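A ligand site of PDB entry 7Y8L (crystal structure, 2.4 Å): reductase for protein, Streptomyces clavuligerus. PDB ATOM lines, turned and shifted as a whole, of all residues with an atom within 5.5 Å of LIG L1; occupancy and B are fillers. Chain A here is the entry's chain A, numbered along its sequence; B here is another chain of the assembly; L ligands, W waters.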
ATOM      1  N   GLY A  11      11.448 -12.476  21.375  1.00  0.00           N
ATOM      2  CA  GLY A  11      11.691 -13.004  20.034  1.00  0.00           C
ATOM      3  C   GLY A  11      10.991 -14.325  19.881  1.00  0.00           C
ATOM      4  O   GLY A  11      11.577 -15.342  20.257  1.00  0.00           O
ATOM      5  N   LEU A  12       9.753 -14.302  19.398  1.00  0.00           N
ATOM      6  CA  LEU A  12       8.947 -15.540  19.349  1.00  0.00           C
ATOM      7  C   LEU A  12       8.667 -15.907  17.903  1.00  0.00           C
ATOM      8  O   LEU A  12       7.521 -16.224  17.578  1.00  0.00           O
ATOM      9  CB  LEU A  12       7.670 -15.332  20.179  1.00  0.00           C
ATOM     10  CG  LEU A  12       7.912 -15.213  21.677  1.00  0.00           C
ATOM     11  CD1 LEU A  12       6.621 -14.929  22.414  1.00  0.00           C
ATOM     12  CD2 LEU A  12       8.571 -16.464  22.217  1.00  0.00           C
ATOM     13  N   GLY A  13       9.705 -15.888  17.086  1.00  0.00           N
ATOM     14  CA  GLY A  13       9.559 -16.391  15.712  1.00  0.00           C
ATOM     15  C   GLY A  13       9.731 -17.889  15.713  1.00  0.00           C
ATOM     16  O   GLY A  13       9.659 -18.515  16.760  1.00  0.00           O
ATOM     17  N   PRO A  14      10.009 -18.548  14.555  1.00  0.00           N
ATOM     18  CA  PRO A  14      10.116 -19.989  14.536  1.00  0.00           C
ATOM     19  C   PRO A  14      10.967 -20.544  15.681  1.00  0.00           C
ATOM     20  O   PRO A  14      10.541 -21.483  16.304  1.00  0.00           O
ATOM     21  CB  PRO A  14      10.927 -20.231  13.249  1.00  0.00           C
ATOM     22  CG  PRO A  14      10.482 -19.181  12.290  1.00  0.00           C
ATOM     23  CD  PRO A  14      10.197 -17.993  13.176  1.00  0.00           C
ATOM     24  N   MET A  15      12.119 -19.935  15.926  1.00  0.00           N
ATOM     25  CA  MET A  15      13.064 -20.448  16.946  1.00  0.00           C
ATOM     26  C   MET A  15      12.589 -20.149  18.353  1.00  0.00           C
ATOM     27  O   MET A  15      12.651 -21.043  19.177  1.00  0.00           O
ATOM     28  CB  MET A  15      14.436 -19.796  16.712  1.00  0.00           C
ATOM     29  CG  MET A  15      15.125 -20.322  15.491  1.00  0.00           C
ATOM     30  SD  MET A  15      15.690 -22.014  15.705  1.00  0.00           S
ATOM     31  CE  MET A  15      17.010 -21.751  16.877  1.00  0.00           C
ATOM     32  N   GLY A  16      12.138 -18.926  18.604  1.00  0.00           N
ATOM     33  CA  GLY A  16      11.737 -18.524  19.963  1.00  0.00           C
ATOM     34  C   GLY A  16      10.504 -19.242  20.467  1.00  0.00           C
ATOM     35  O   GLY A  16      10.456 -19.548  21.628  1.00  0.00           O
ATOM     36  N   TRP A  33       7.716 -12.164  25.645  1.00  0.00           N
ATOM     37  CA  TRP A  33       7.335 -10.885  25.020  1.00  0.00           C
ATOM     38  C   TRP A  33       7.691 -10.963  23.537  1.00  0.00           C
ATOM     39  O   TRP A  33       8.793 -11.426  23.235  1.00  0.00           O
ATOM     40  CB  TRP A  33       7.980  -9.666  25.680  1.00  0.00           C
ATOM     41  CG  TRP A  33       7.272  -8.410  25.267  1.00  0.00           C
ATOM     42  CD1 TRP A  33       6.184  -7.847  25.864  1.00  0.00           C
ATOM     43  CD2 TRP A  33       7.551  -7.593  24.117  1.00  0.00           C
ATOM     44  NE1 TRP A  33       5.784  -6.728  25.184  1.00  0.00           N
ATOM     45  CE2 TRP A  33       6.613  -6.553  24.105  1.00  0.00           C
ATOM     46  CE3 TRP A  33       8.517  -7.637  23.101  1.00  0.00           C
ATOM     47  CZ2 TRP A  33       6.607  -5.560  23.127  1.00  0.00           C
ATOM     48  CZ3 TRP A  33       8.509  -6.660  22.141  1.00  0.00           C
ATOM     49  CH2 TRP A  33       7.566  -5.629  22.159  1.00  0.00           C
ATOM     50  N   ASN A  34       6.770 -10.564  22.687  1.00  0.00           N
ATOM     51  CA  ASN A  34       7.073 -10.488  21.240  1.00  0.00           C
ATOM     52  C   ASN A  34       6.399  -9.249  20.676  1.00  0.00           C
ATOM     53  O   ASN A  34       5.339  -8.861  21.182  1.00  0.00           O
ATOM     54  CB  ASN A  34       6.641 -11.723  20.459  1.00  0.00           C
ATOM     55  CG  ASN A  34       7.306 -11.796  19.102  1.00  0.00           C
ATOM     56  OD1 ASN A  34       8.511 -11.612  18.988  1.00  0.00           O
ATOM     57  ND2 ASN A  34       6.521 -12.031  18.070  1.00  0.00           N
ATOM     58  N   ARG A  35       7.019  -8.639  19.671  1.00  0.00           N
ATOM     59  CA  ARG A  35       6.447  -7.442  19.011  1.00  0.00           C
ATOM     60  C   ARG A  35       5.100  -7.851  18.431  1.00  0.00           C
ATOM     61  O   ARG A  35       4.116  -7.192  18.771  1.00  0.00           O
ATOM     62  CB  ARG A  35       7.483  -6.935  18.009  1.00  0.00           C
ATOM     63  CG  ARG A  35       7.216  -5.563  17.414  1.00  0.00           C
ATOM     64  CD  ARG A  35       8.323  -5.210  16.433  1.00  0.00           C
ATOM     65  NE  ARG A  35       8.736  -6.352  15.618  1.00  0.00           N
ATOM     66  CZ  ARG A  35       9.563  -6.277  14.581  1.00  0.00           C
ATOM     67  NH1 ARG A  35      10.093  -5.114  14.231  1.00  0.00           N
ATOM     68  NH2 ARG A  35       9.878  -7.369  13.902  1.00  0.00           N
ATOM     69  N   THR A  36       5.069  -8.899  17.618  1.00  0.00           N
ATOM     70  CA  THR A  36       3.761  -9.433  17.144  1.00  0.00           C
ATOM     71  C   THR A  36       3.177 -10.254  18.287  1.00  0.00           C
ATOM     72  O   THR A  36       3.555 -11.423  18.435  1.00  0.00           O
ATOM     73  CB  THR A  36       3.910 -10.148  15.793  1.00  0.00           C
ATOM     74  OG1 THR A  36       4.487  -9.213  14.877  1.00  0.00           O
ATOM     75  CG2 THR A  36       2.593 -10.644  15.241  1.00  0.00           C
ATOM     76  N   ARG A  39       1.990 -14.201  18.705  1.00  0.00           N
ATOM     77  CA  ARG A  39       2.924 -15.352  18.731  1.00  0.00           C
ATOM     78  C   ARG A  39       3.132 -15.833  20.163  1.00  0.00           C
ATOM     79  O   ARG A  39       3.488 -16.997  20.335  1.00  0.00           O
ATOM     80  CB  ARG A  39       4.200 -14.874  18.043  1.00  0.00           C
ATOM     81  CG  ARG A  39       3.975 -14.499  16.585  1.00  0.00           C
ATOM     82  CD  ARG A  39       5.258 -14.198  15.852  1.00  0.00           C
ATOM     83  NE  ARG A  39       5.651 -15.266  14.952  1.00  0.00           N
ATOM     84  CZ  ARG A  39       6.596 -15.157  14.025  1.00  0.00           C
ATOM     85  NH1 ARG A  39       7.238 -14.006  13.887  1.00  0.00           N
ATOM     86  NH2 ARG A  39       6.887 -16.180  13.246  1.00  0.00           N
ATOM     87  N   SER A  67      15.853 -13.985  20.751  1.00  0.00           N
ATOM     88  CA  SER A  67      15.896 -14.720  19.466  1.00  0.00           C
ATOM     89  C   SER A  67      15.365 -13.777  18.382  1.00  0.00           C
ATOM     90  O   SER A  67      14.195 -13.868  18.024  1.00  0.00           O
ATOM     91  CB  SER A  67      15.154 -16.028  19.504  1.00  0.00           C
ATOM     92  OG  SER A  67      15.331 -16.740  18.288  1.00  0.00           O
ATOM     93  N   LEU A  68      16.231 -12.889  17.908  1.00  0.00           N
ATOM     94  CA  LEU A  68      15.846 -11.898  16.884  1.00  0.00           C
ATOM     95  C   LEU A  68      16.678 -12.116  15.615  1.00  0.00           C
ATOM     96  O   LEU A  68      17.613 -12.866  15.682  1.00  0.00           O
ATOM     97  CB  LEU A  68      16.057 -10.500  17.480  1.00  0.00           C
ATOM     98  CG  LEU A  68      15.600 -10.312  18.926  1.00  0.00           C
ATOM     99  CD1 LEU A  68      16.261  -9.103  19.545  1.00  0.00           C
ATOM    100  CD2 LEU A  68      14.083 -10.193  19.009  1.00  0.00           C
ATOM    101  N   THR A  69      16.353 -11.456  14.509  1.00  0.00           N
ATOM    102  CA  THR A  69      17.033 -11.665  13.206  1.00  0.00           C
ATOM    103  C   THR A  69      18.510 -11.285  13.262  1.00  0.00           C
ATOM    104  O   THR A  69      19.306 -11.955  12.614  1.00  0.00           O
ATOM    105  CB  THR A  69      16.352 -10.855  12.096  1.00  0.00           C
ATOM    106  OG1 THR A  69      14.959 -10.762  12.335  1.00  0.00           O
ATOM    107  CG2 THR A  69      16.595 -11.411  10.713  1.00  0.00           C
ATOM    108  N   ASP A  70      18.832 -10.247  14.034  1.00  0.00           N
ATOM    109  CA  ASP A  70      20.224  -9.745  14.076  1.00  0.00           C
ATOM    110  C   ASP A  70      20.464  -8.939  15.338  1.00  0.00           C
ATOM    111  O   ASP A  70      19.570  -8.879  16.187  1.00  0.00           O
ATOM    112  CB  ASP A  70      20.564  -8.930  12.818  1.00  0.00           C
ATOM    113  CG  ASP A  70      19.577  -7.874  12.371  1.00  0.00           C
ATOM    114  OD1 ASP A  70      18.855  -7.342  13.210  1.00  0.00           O
ATOM    115  OD2 ASP A  70      19.550  -7.587  11.163  1.00  0.00           O
ATOM    116  N   ASP A  72      21.085  -5.685  15.309  1.00  0.00           N
ATOM    117  CA  ASP A  72      20.444  -4.369  15.103  1.00  0.00           C
ATOM    118  C   ASP A  72      19.047  -4.409  15.703  1.00  0.00           C
ATOM    119  O   ASP A  72      18.618  -3.400  16.260  1.00  0.00           O
ATOM    120  CB  ASP A  72      20.406  -3.977  13.624  1.00  0.00           C
ATOM    121  CG  ASP A  72      21.690  -3.361  13.120  1.00  0.00           C
ATOM    122  OD1 ASP A  72      22.173  -2.416  13.766  1.00  0.00           O
ATOM    123  OD2 ASP A  72      22.186  -3.820  12.080  1.00  0.00           O
ATOM    124  N   ALA A  73      18.373  -5.552  15.578  1.00  0.00           N
ATOM    125  CA  ALA A  73      17.044  -5.741  16.187  1.00  0.00           C
ATOM    126  C   ALA A  73      17.111  -5.590  17.713  1.00  0.00           C
ATOM    127  O   ALA A  73      16.153  -5.056  18.257  1.00  0.00           O
ATOM    128  CB  ALA A  73      16.587  -7.102  15.816  1.00  0.00           C
ATOM    129  N   ALA A  76      17.060  -1.885  18.683  1.00  0.00           N
ATOM    130  CA  ALA A  76      15.750  -1.220  18.466  1.00  0.00           C
ATOM    131  C   ALA A  76      14.716  -1.673  19.496  1.00  0.00           C
ATOM    132  O   ALA A  76      13.788  -0.918  19.752  1.00  0.00           O
ATOM    133  CB  ALA A  76      15.307  -1.519  17.065  1.00  0.00           C
ATOM    134  N   LEU A  77      14.888  -2.856  20.066  1.00  0.00           N
ATOM    135  CA  LEU A  77      13.918  -3.418  21.020  1.00  0.00           C
ATOM    136  C   LEU A  77      14.340  -3.104  22.448  1.00  0.00           C
ATOM    137  O   LEU A  77      13.491  -2.660  23.216  1.00  0.00           O
ATOM    138  CB  LEU A  77      13.903  -4.930  20.783  1.00  0.00           C
ATOM    139  CG  LEU A  77      12.897  -5.722  21.582  1.00  0.00           C
ATOM    140  CD1 LEU A  77      11.517  -5.113  21.429  1.00  0.00           C
ATOM    141  CD2 LEU A  77      12.898  -7.158  21.116  1.00  0.00           C
ATOM    142  N   LEU A  93      20.696 -15.101  21.163  1.00  0.00           N
ATOM    143  CA  LEU A  93      20.827 -16.254  20.259  1.00  0.00           C
ATOM    144  C   LEU A  93      20.597 -15.770  18.827  1.00  0.00           C
ATOM    145  O   LEU A  93      20.183 -16.585  17.995  1.00  0.00           O
ATOM    146  CB  LEU A  93      19.816 -17.306  20.701  1.00  0.00           C
ATOM    147  CG  LEU A  93      19.986 -17.803  22.130  1.00  0.00           C
ATOM    148  CD1 LEU A  93      19.015 -18.924  22.446  1.00  0.00           C
ATOM    149  CD2 LEU A  93      21.405 -18.271  22.356  1.00  0.00           C
ATOM    150  N   SER A  94      20.895 -14.513  18.563  1.00  0.00           N
ATOM    151  CA  SER A  94      20.721 -13.936  17.212  1.00  0.00           C
ATOM    152  C   SER A  94      22.015 -13.996  16.410  1.00  0.00           C
ATOM    153  O   SER A  94      23.063 -13.681  16.962  1.00  0.00           O
ATOM    154  CB  SER A  94      20.193 -12.517  17.286  1.00  0.00           C
ATOM    155  OG  SER A  94      19.135 -12.403  18.223  1.00  0.00           O
ATOM    156  N   SER A  95      21.915 -14.417  15.154  1.00  0.00           N
ATOM    157  CA  SER A  95      23.070 -14.432  14.239  1.00  0.00           C
ATOM    158  C   SER A  95      23.521 -13.016  13.892  1.00  0.00           C
ATOM    159  O   SER A  95      22.647 -12.161  13.711  1.00  0.00           O
ATOM    160  CB  SER A  95      22.768 -15.153  12.966  1.00  0.00           C
ATOM    161  OG  SER A  95      23.882 -15.132  12.085  1.00  0.00           O
ATOM    162  N   VAL A 120      22.777 -20.943  17.780  1.00  0.00           N
ATOM    163  CA  VAL A 120      22.029 -22.228  17.845  1.00  0.00           C
ATOM    164  C   VAL A 120      22.219 -22.972  16.534  1.00  0.00           C
ATOM    165  O   VAL A 120      21.713 -22.513  15.519  1.00  0.00           O
ATOM    166  CB  VAL A 120      20.550 -22.028  18.207  1.00  0.00           C
ATOM    167  CG1 VAL A 120      19.927 -23.306  18.709  1.00  0.00           C
ATOM    168  CG2 VAL A 120      20.366 -20.908  19.226  1.00  0.00           C
ATOM    169  N   THR A 121      22.937 -24.083  16.580  1.00  0.00           N
ATOM    170  CA  THR A 121      23.172 -24.906  15.390  1.00  0.00           C
ATOM    171  C   THR A 121      22.069 -25.948  15.336  1.00  0.00           C
ATOM    172  O   THR A 121      22.402 -27.098  15.040  1.00  0.00           O
ATOM    173  CB  THR A 121      24.592 -25.474  15.411  1.00  0.00           C
ATOM    174  OG1 THR A 121      24.765 -26.286  16.579  1.00  0.00           O
ATOM    175  CG2 THR A 121      25.653 -24.408  15.378  1.00  0.00           C
ATOM    176  N   CYS A 122      20.839 -25.588  15.704  1.00  0.00           N
ATOM    177  CA  CYS A 122      19.669 -26.514  15.644  1.00  0.00           C
ATOM    178  C   CYS A 122      18.464 -25.808  14.991  1.00  0.00           C
ATOM    179  O   CYS A 122      18.323 -24.589  15.143  1.00  0.00           O
ATOM    180  CB  CYS A 122      19.301 -27.067  17.018  1.00  0.00           C
ATOM    181  SG  CYS A 122      18.131 -26.097  17.976  1.00  0.00           S
ATOM    182  N   PRO A 123      17.673 -26.497  14.137  1.00  0.00           N
ATOM    183  CA  PRO A 123      16.468 -25.910  13.581  1.00  0.00           C
ATOM    184  C   PRO A 123      15.442 -25.727  14.708  1.00  0.00           C
ATOM    185  O   PRO A 123      15.683 -26.181  15.800  1.00  0.00           O
ATOM    186  CB  PRO A 123      15.992 -26.979  12.609  1.00  0.00           C
ATOM    187  CG  PRO A 123      16.459 -28.254  13.224  1.00  0.00           C
ATOM    188  CD  PRO A 123      17.836 -27.902  13.711  1.00  0.00           C
ATOM    189  N   PRO A 124      14.252 -25.075  14.519  1.00  0.00           N
ATOM    190  CA  PRO A 124      13.277 -24.989  15.601  1.00  0.00           C
ATOM    191  C   PRO A 124      12.841 -26.394  16.066  1.00  0.00           C
ATOM    192  O   PRO A 124      12.617 -26.552  17.228  1.00  0.00           O
ATOM    193  CB  PRO A 124      12.134 -24.181  14.999  1.00  0.00           C
ATOM    194  CG  PRO A 124      12.773 -23.361  13.933  1.00  0.00           C
ATOM    195  CD  PRO A 124      13.751 -24.333  13.326  1.00  0.00           C
ATOM    196  N   TYR A 170      29.496 -20.085  14.530  1.00  0.00           N
ATOM    197  CA  TYR A 170      28.186 -20.208  13.849  1.00  0.00           C
ATOM    198  C   TYR A 170      28.355 -19.929  12.348  1.00  0.00           C
ATOM    199  O   TYR A 170      27.794 -20.691  11.566  1.00  0.00           O
ATOM    200  CB  TYR A 170      27.153 -19.286  14.493  1.00  0.00           C
ATOM    201  CG  TYR A 170      25.780 -19.375  13.892  1.00  0.00           C
ATOM    202  CD1 TYR A 170      24.916 -20.391  14.238  1.00  0.00           C
ATOM    203  CD2 TYR A 170      25.352 -18.446  12.968  1.00  0.00           C
ATOM    204  CE1 TYR A 170      23.654 -20.499  13.681  1.00  0.00           C
ATOM    205  CE2 TYR A 170      24.092 -18.528  12.397  1.00  0.00           C
ATOM    206  CZ  TYR A 170      23.241 -19.550  12.760  1.00  0.00           C
ATOM    207  OH  TYR A 170      22.005 -19.625  12.192  1.00  0.00           O
ATOM    208  N   ALA B 232       9.262 -22.216   9.208  1.00  0.00           N
ATOM    209  CA  ALA B 232      10.542 -22.614   9.835  1.00  0.00           C
ATOM    210  C   ALA B 232      11.633 -21.584   9.525  1.00  0.00           C
ATOM    211  O   ALA B 232      12.568 -21.481  10.333  1.00  0.00           O
ATOM    212  CB  ALA B 232      10.938 -23.990   9.370  1.00  0.00           C
ATOM    213  N   ASP B 233      11.505 -20.855   8.431  1.00  0.00           N
ATOM    214  CA  ASP B 233      12.544 -19.874   8.032  1.00  0.00           C
ATOM    215  C   ASP B 233      11.966 -18.804   7.122  1.00  0.00           C
ATOM    216  O   ASP B 233      11.067 -19.110   6.336  1.00  0.00           O
ATOM    217  CB  ASP B 233      13.697 -20.574   7.316  1.00  0.00           C
ATOM    218  CG  ASP B 233      13.417 -20.865   5.867  1.00  0.00           C
ATOM    219  OD1 ASP B 233      13.885 -20.093   5.033  1.00  0.00           O
ATOM    220  OD2 ASP B 233      12.700 -21.837   5.599  1.00  0.00           O
ATOM    221  N   ARG B 234      12.421 -17.572   7.279  1.00  0.00           N
ATOM    222  CA  ARG B 234      12.030 -16.482   6.372  1.00  0.00           C
ATOM    223  C   ARG B 234      13.276 -16.143   5.571  1.00  0.00           C
ATOM    224  O   ARG B 234      14.368 -16.152   6.153  1.00  0.00           O
ATOM    225  CB  ARG B 234      11.527 -15.266   7.157  1.00  0.00           C
ATOM    226  CG  ARG B 234      10.230 -15.456   7.913  1.00  0.00           C
ATOM    227  CD  ARG B 234       9.854 -14.151   8.582  1.00  0.00           C
ATOM    228  NE  ARG B 234      10.982 -13.505   9.258  1.00  0.00           N
ATOM    229  CZ  ARG B 234      11.421 -12.274   9.018  1.00  0.00           C
ATOM    230  NH1 ARG B 234      10.837 -11.520   8.100  1.00  0.00           N
ATOM    231  NH2 ARG B 234      12.456 -11.806   9.688  1.00  0.00           N
ATOM    232  N   MET B 237      15.548 -13.511   7.008  1.00  0.00           N
ATOM    233  CA  MET B 237      16.432 -13.939   8.112  1.00  0.00           C
ATOM    234  C   MET B 237      17.643 -14.642   7.510  1.00  0.00           C
ATOM    235  O   MET B 237      18.728 -14.480   8.064  1.00  0.00           O
ATOM    236  CB  MET B 237      15.691 -14.856   9.095  1.00  0.00           C
ATOM    237  CG  MET B 237      16.582 -15.487  10.135  1.00  0.00           C
ATOM    238  SD  MET B 237      17.135 -17.134   9.660  1.00  0.00           S
ATOM    239  CE  MET B 237      15.558 -17.906   9.322  1.00  0.00           C
ATOM    240  N   SER B 241      21.609 -13.828   7.400  1.00  0.00           N
ATOM    241  CA  SER B 241      22.591 -14.886   7.761  1.00  0.00           C
ATOM    242  C   SER B 241      23.710 -15.012   6.713  1.00  0.00           C
ATOM    243  O   SER B 241      24.860 -15.176   7.108  1.00  0.00           O
ATOM    244  CB  SER B 241      21.902 -16.221   7.986  1.00  0.00           C
ATOM    245  OG  SER B 241      22.802 -17.173   8.532  1.00  0.00           O
HETATM  246  P1  LIG L   1      13.063 -14.456  12.474  1.00  0.00           P
HETATM  247  O1  LIG L   1      13.844 -13.363  11.868  1.00  0.00           O
HETATM  248  O2  LIG L   1      12.101 -15.211  11.625  1.00  0.00           O
HETATM  249  O3  LIG L   1      12.286 -13.913  13.769  1.00  0.00           O
HETATM  250  C1  LIG L   1      13.055 -13.550  14.933  1.00  0.00           C
HETATM  251  C2  LIG L   1      12.269 -12.600  15.817  1.00  0.00           C
HETATM  252  O4  LIG L   1      12.906 -11.306  15.822  1.00  0.00           O
HETATM  253  C3  LIG L   1      10.794 -12.339  15.468  1.00  0.00           C
HETATM  254  O5  LIG L   1       9.974 -12.890  16.496  1.00  0.00           O
HETATM  255  C4  LIG L   1      10.678 -10.812  15.365  1.00  0.00           C
HETATM  256  O6  LIG L   1       9.511 -10.312  16.018  1.00  0.00           O
HETATM  257  C5  LIG L   1      11.920 -10.356  16.123  1.00  0.00           C
HETATM  258  N1  LIG L   1      12.418  -9.037  15.763  1.00  0.00           N
HETATM  259  C6  LIG L   1      13.184  -8.711  14.666  1.00  0.00           C
HETATM  260  N2  LIG L   1      13.499  -7.434  14.617  1.00  0.00           N
HETATM  261  C7  LIG L   1      12.924  -6.893  15.753  1.00  0.00           C
HETATM  262  C8  LIG L   1      12.893  -5.589  16.272  1.00  0.00           C
HETATM  263  N3  LIG L   1      13.497  -4.558  15.691  1.00  0.00           N
HETATM  264  N4  LIG L   1      12.225  -5.383  17.428  1.00  0.00           N
HETATM  265  C9  LIG L   1      11.621  -6.424  18.006  1.00  0.00           C
HETATM  266  N5  LIG L   1      11.579  -7.697  17.608  1.00  0.00           N
HETATM  267  C10 LIG L   1      12.250  -7.874  16.461  1.00  0.00           C
HETATM  268  O7  LIG L   1      14.114 -15.473  13.097  1.00  0.00           O
HETATM  269  P2  LIG L   1      14.099 -17.013  13.536  1.00  0.00           P
HETATM  270  O8  LIG L   1      13.112 -17.187  14.634  1.00  0.00           O
HETATM  271  O9  LIG L   1      13.982 -17.847  12.311  1.00  0.00           O
HETATM  272  O10 LIG L   1      15.577 -17.144  14.123  1.00  0.00           O
HETATM  273  C11 LIG L   1      16.073 -16.136  15.018  1.00  0.00           C
HETATM  274  C12 LIG L   1      17.580 -16.100  14.949  1.00  0.00           C
HETATM  275  O11 LIG L   1      18.100 -17.447  15.103  1.00  0.00           O
HETATM  276  C13 LIG L   1      18.178 -15.545  13.646  1.00  0.00           C
HETATM  277  O12 LIG L   1      19.270 -14.685  13.926  1.00  0.00           O
HETATM  278  C14 LIG L   1      18.590 -16.807  12.903  1.00  0.00           C
HETATM  279  O13 LIG L   1      19.699 -16.603  12.047  1.00  0.00           O
HETATM  280  C15 LIG L   1      18.925 -17.772  14.025  1.00  0.00           C
HETATM  281  N6  LIG L   1      18.691 -19.192  13.656  1.00  0.00           N
HETATM  282  C16 LIG L   1      17.607 -19.571  12.901  1.00  0.00           C
HETATM  283  C17 LIG L   1      17.304 -20.895  12.709  1.00  0.00           C
HETATM  284  C18 LIG L   1      16.094 -21.273  11.931  1.00  0.00           C
HETATM  285  O14 LIG L   1      15.226 -20.443  11.699  1.00  0.00           O
HETATM  286  N7  LIG L   1      16.000 -22.529  11.532  1.00  0.00           N
HETATM  287  C19 LIG L   1      18.177 -21.929  13.287  1.00  0.00           C
HETATM  288  C20 LIG L   1      19.234 -21.398  14.139  1.00  0.00           C
HETATM  289  C21 LIG L   1      19.577 -20.147  14.063  1.00  0.00           C
HETATM  290  P3  LIG L   1       8.203 -10.286  15.085  1.00  0.00           P
HETATM  291  O15 LIG L   1       8.653 -10.191  13.654  1.00  0.00           O
HETATM  292  O16 LIG L   1       7.475  -9.057  15.536  1.00  0.00           O
HETATM  293  O17 LIG L   1       7.377 -11.514  15.323  1.00  0.00           O
HETATM  294  C1  LG2 L   2      19.367 -25.506  10.397  1.00  0.00           C
HETATM  295  C2  LG2 L   2      20.615 -26.143  10.928  1.00  0.00           C
HETATM  296  C3  LG2 L   2      19.619 -24.156  10.497  1.00  0.00           C
HETATM  297  C4  LG2 L   2      21.084 -25.135  11.926  1.00  0.00           C
HETATM  298  C5  LG2 L   2      18.988 -23.202   9.820  1.00  0.00           C
HETATM  299  C6  LG2 L   2      19.380 -21.884   9.966  1.00  0.00           C
HETATM  300  C7  LG2 L   2      17.934 -23.511   8.972  1.00  0.00           C
HETATM  301  C8  LG2 L   2      17.282 -22.504   8.274  1.00  0.00           C
HETATM  302  C9  LG2 L   2      18.734 -20.873   9.284  1.00  0.00           C
HETATM  303  C10 LG2 L   2      17.694 -21.182   8.432  1.00  0.00           C
HETATM  304  F1  LG2 L   2      20.363 -21.597  10.781  1.00  0.00           F
HETATM  305  F2  LG2 L   2      16.314 -22.779   7.482  1.00  0.00           F
HETATM  306  N1  LG2 L   2      20.592 -23.879  11.375  1.00  0.00           N
HETATM  307  O   HOH W   1       9.976  -9.452  10.969  1.00  0.00           O
HETATM  308  O   HOH W   2      12.807 -17.131  10.123  1.00  0.00           O
HETATM  309  O   HOH W   3      19.603 -14.069  10.513  1.00  0.00           O
HETATM  310  O   HOH W   4      21.331 -18.408  16.366  1.00  0.00           O
HETATM  311  O   HOH W   5       9.443 -14.559  12.161  1.00  0.00           O
HETATM  312  O   HOH W   6       6.613  -8.797  11.926  1.00  0.00           O
HETATM  313  O   HOH W   7      17.703 -18.158  17.853  1.00  0.00           O
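NE of Arg 39 lies within hydrogen-bond range of O of Leu 12, 3.4 Å away. The side-chain amide nitrogen of Asn 34 is in hydrogen-bond range of the backbone carbonyl oxygen of Thr 36, at 3.0 Å. N of Leu 12 is in hydrogen-bond range of OD1 of Asn 34, at 3.0 Å. The backbone NH (N) of Leu 68 sits at hydrogen-bond distance from the side-chain hydroxyl (OG) of Ser 94. N of Ala 73 lies within hydrogen-bond range of OD1 of Asp 70, 3.0 Å away. N of Gly 11 is in hydrogen-bond range of O of Trp 33.
The backbone nitrogen (N) of Pro 14 sits close to an oxygen (O8) of LIG L1. An oxygen (O14) of LIG L1 lies close to the backbone carbonyl oxygen of Ala 232 of chain B (3.2 Å). Gly 11 touches LIG L1. Ser 67 touches LIG L1. Ala 73 touches LIG L1 (CB to N2, 3.3 Å). Ala 76 touches LIG L1 (CB to N3, 3.8 Å). CD2 of Leu 77 touches C9 of LIG L1, 3.4 Å away. O of Leu 93 touches O11 of LIG L1, at 3.7 Å. Ser 94 touches LIG L1. Val 120 touches LIG L1 (O to C20, 3.0 Å). Cys 122 touches LIG L1 (O to C19, 3.2 Å). Pro 123 touches LIG L1 (CA to N7, 3.98 Å). CD of Pro 124 touches N7 of LIG L1, at 3.4 Å. Tyr 170 touches LIG L1. Hydrophobic or aromatic side chains that line LIG L1: Pro 14, Met 15, Leu 68, Ala 73, Ala 76, Leu 77, Pro 124, Tyr 170 and Met 237 of chain B. The nearest printed residue that does not touch LIG L1 is Gly 16 (4.4 Å).
O12 of LIG L1 sits at hydrogen-bond distance from O of Thr 69. The side-chain hydroxyl (OG1) of Thr 69 lies within hydrogen-bond range of an oxygen (O1) of LIG L1 (2.9 Å). NH1 of Arg 39 lies within salt-bridge range of O17 of LIG L1. The side-chain amide nitrogen (ND2) of Asn 34 is in hydrogen-bond range of an oxygen (O17) of LIG L1 (2.9 Å). The backbone NH of Ser 95 is in hydrogen-bond range of an oxygen (O12) of LIG L1. NE of Arg 35 is in salt-bridge range of O16 of LIG L1. The guanidinium group (NH2) of Arg 234 of chain B is in salt-bridge range of an oxygen (O1) of LIG L1 (3.0 Å). An oxygen (O12) of LIG L1 lies within hydrogen-bond range of the backbone carbonyl oxygen (O) of Leu 68, at 3.0 Å. An oxygen (O16) of LIG L1 lies within hydrogen-bond range of the backbone NH (N) of Thr 36, 3.2 Å away. The side-chain hydroxyl (OG1) of Thr 36 lies within hydrogen-bond range of an oxygen (O16) of LIG L1, 3.1 Å away. N of Gly 13 lies within hydrogen-bond range of O5 of LIG L1 (3.1 Å). O8 of LIG L1 is in hydrogen-bond range of N of Met 15. N of Leu 12 sits at hydrogen-bond distance from O5 of LIG L1 (3.2 Å). The side-chain sulfur of Met 237 of chain B is in hydrogen-bond range of an oxygen (O13) of LIG L1 (3.5 Å).
Water W2 bridges an oxygen (O2) of LIG L1 and the backbone NH of Arg 234 of chain B. Water W5 lies within hydrogen-bond range of an oxygen (O2) of LIG L1 (2.8 Å), the guanidinium group of Arg 39 (2.9 Å) and the guanidinium group of Arg 234 of chain B (3.5 Å). Water W7 lies within hydrogen-bond range of OG of Ser 67 (2.8 Å), O11 of LIG L1 (2.9 Å) and O of Leu 93 (2.9 Å). Water W3 lies within hydrogen-bond range of the backbone carbonyl oxygen (O) of Met 237 of chain B (2.6 Å), an oxygen (O13) of LIG L1 (3.0 Å) and the backbone carbonyl oxygen (O) of Thr 69 (3.0 Å). Water W4 lies within hydrogen-bond range of O of Leu 93 and N of Val 120.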
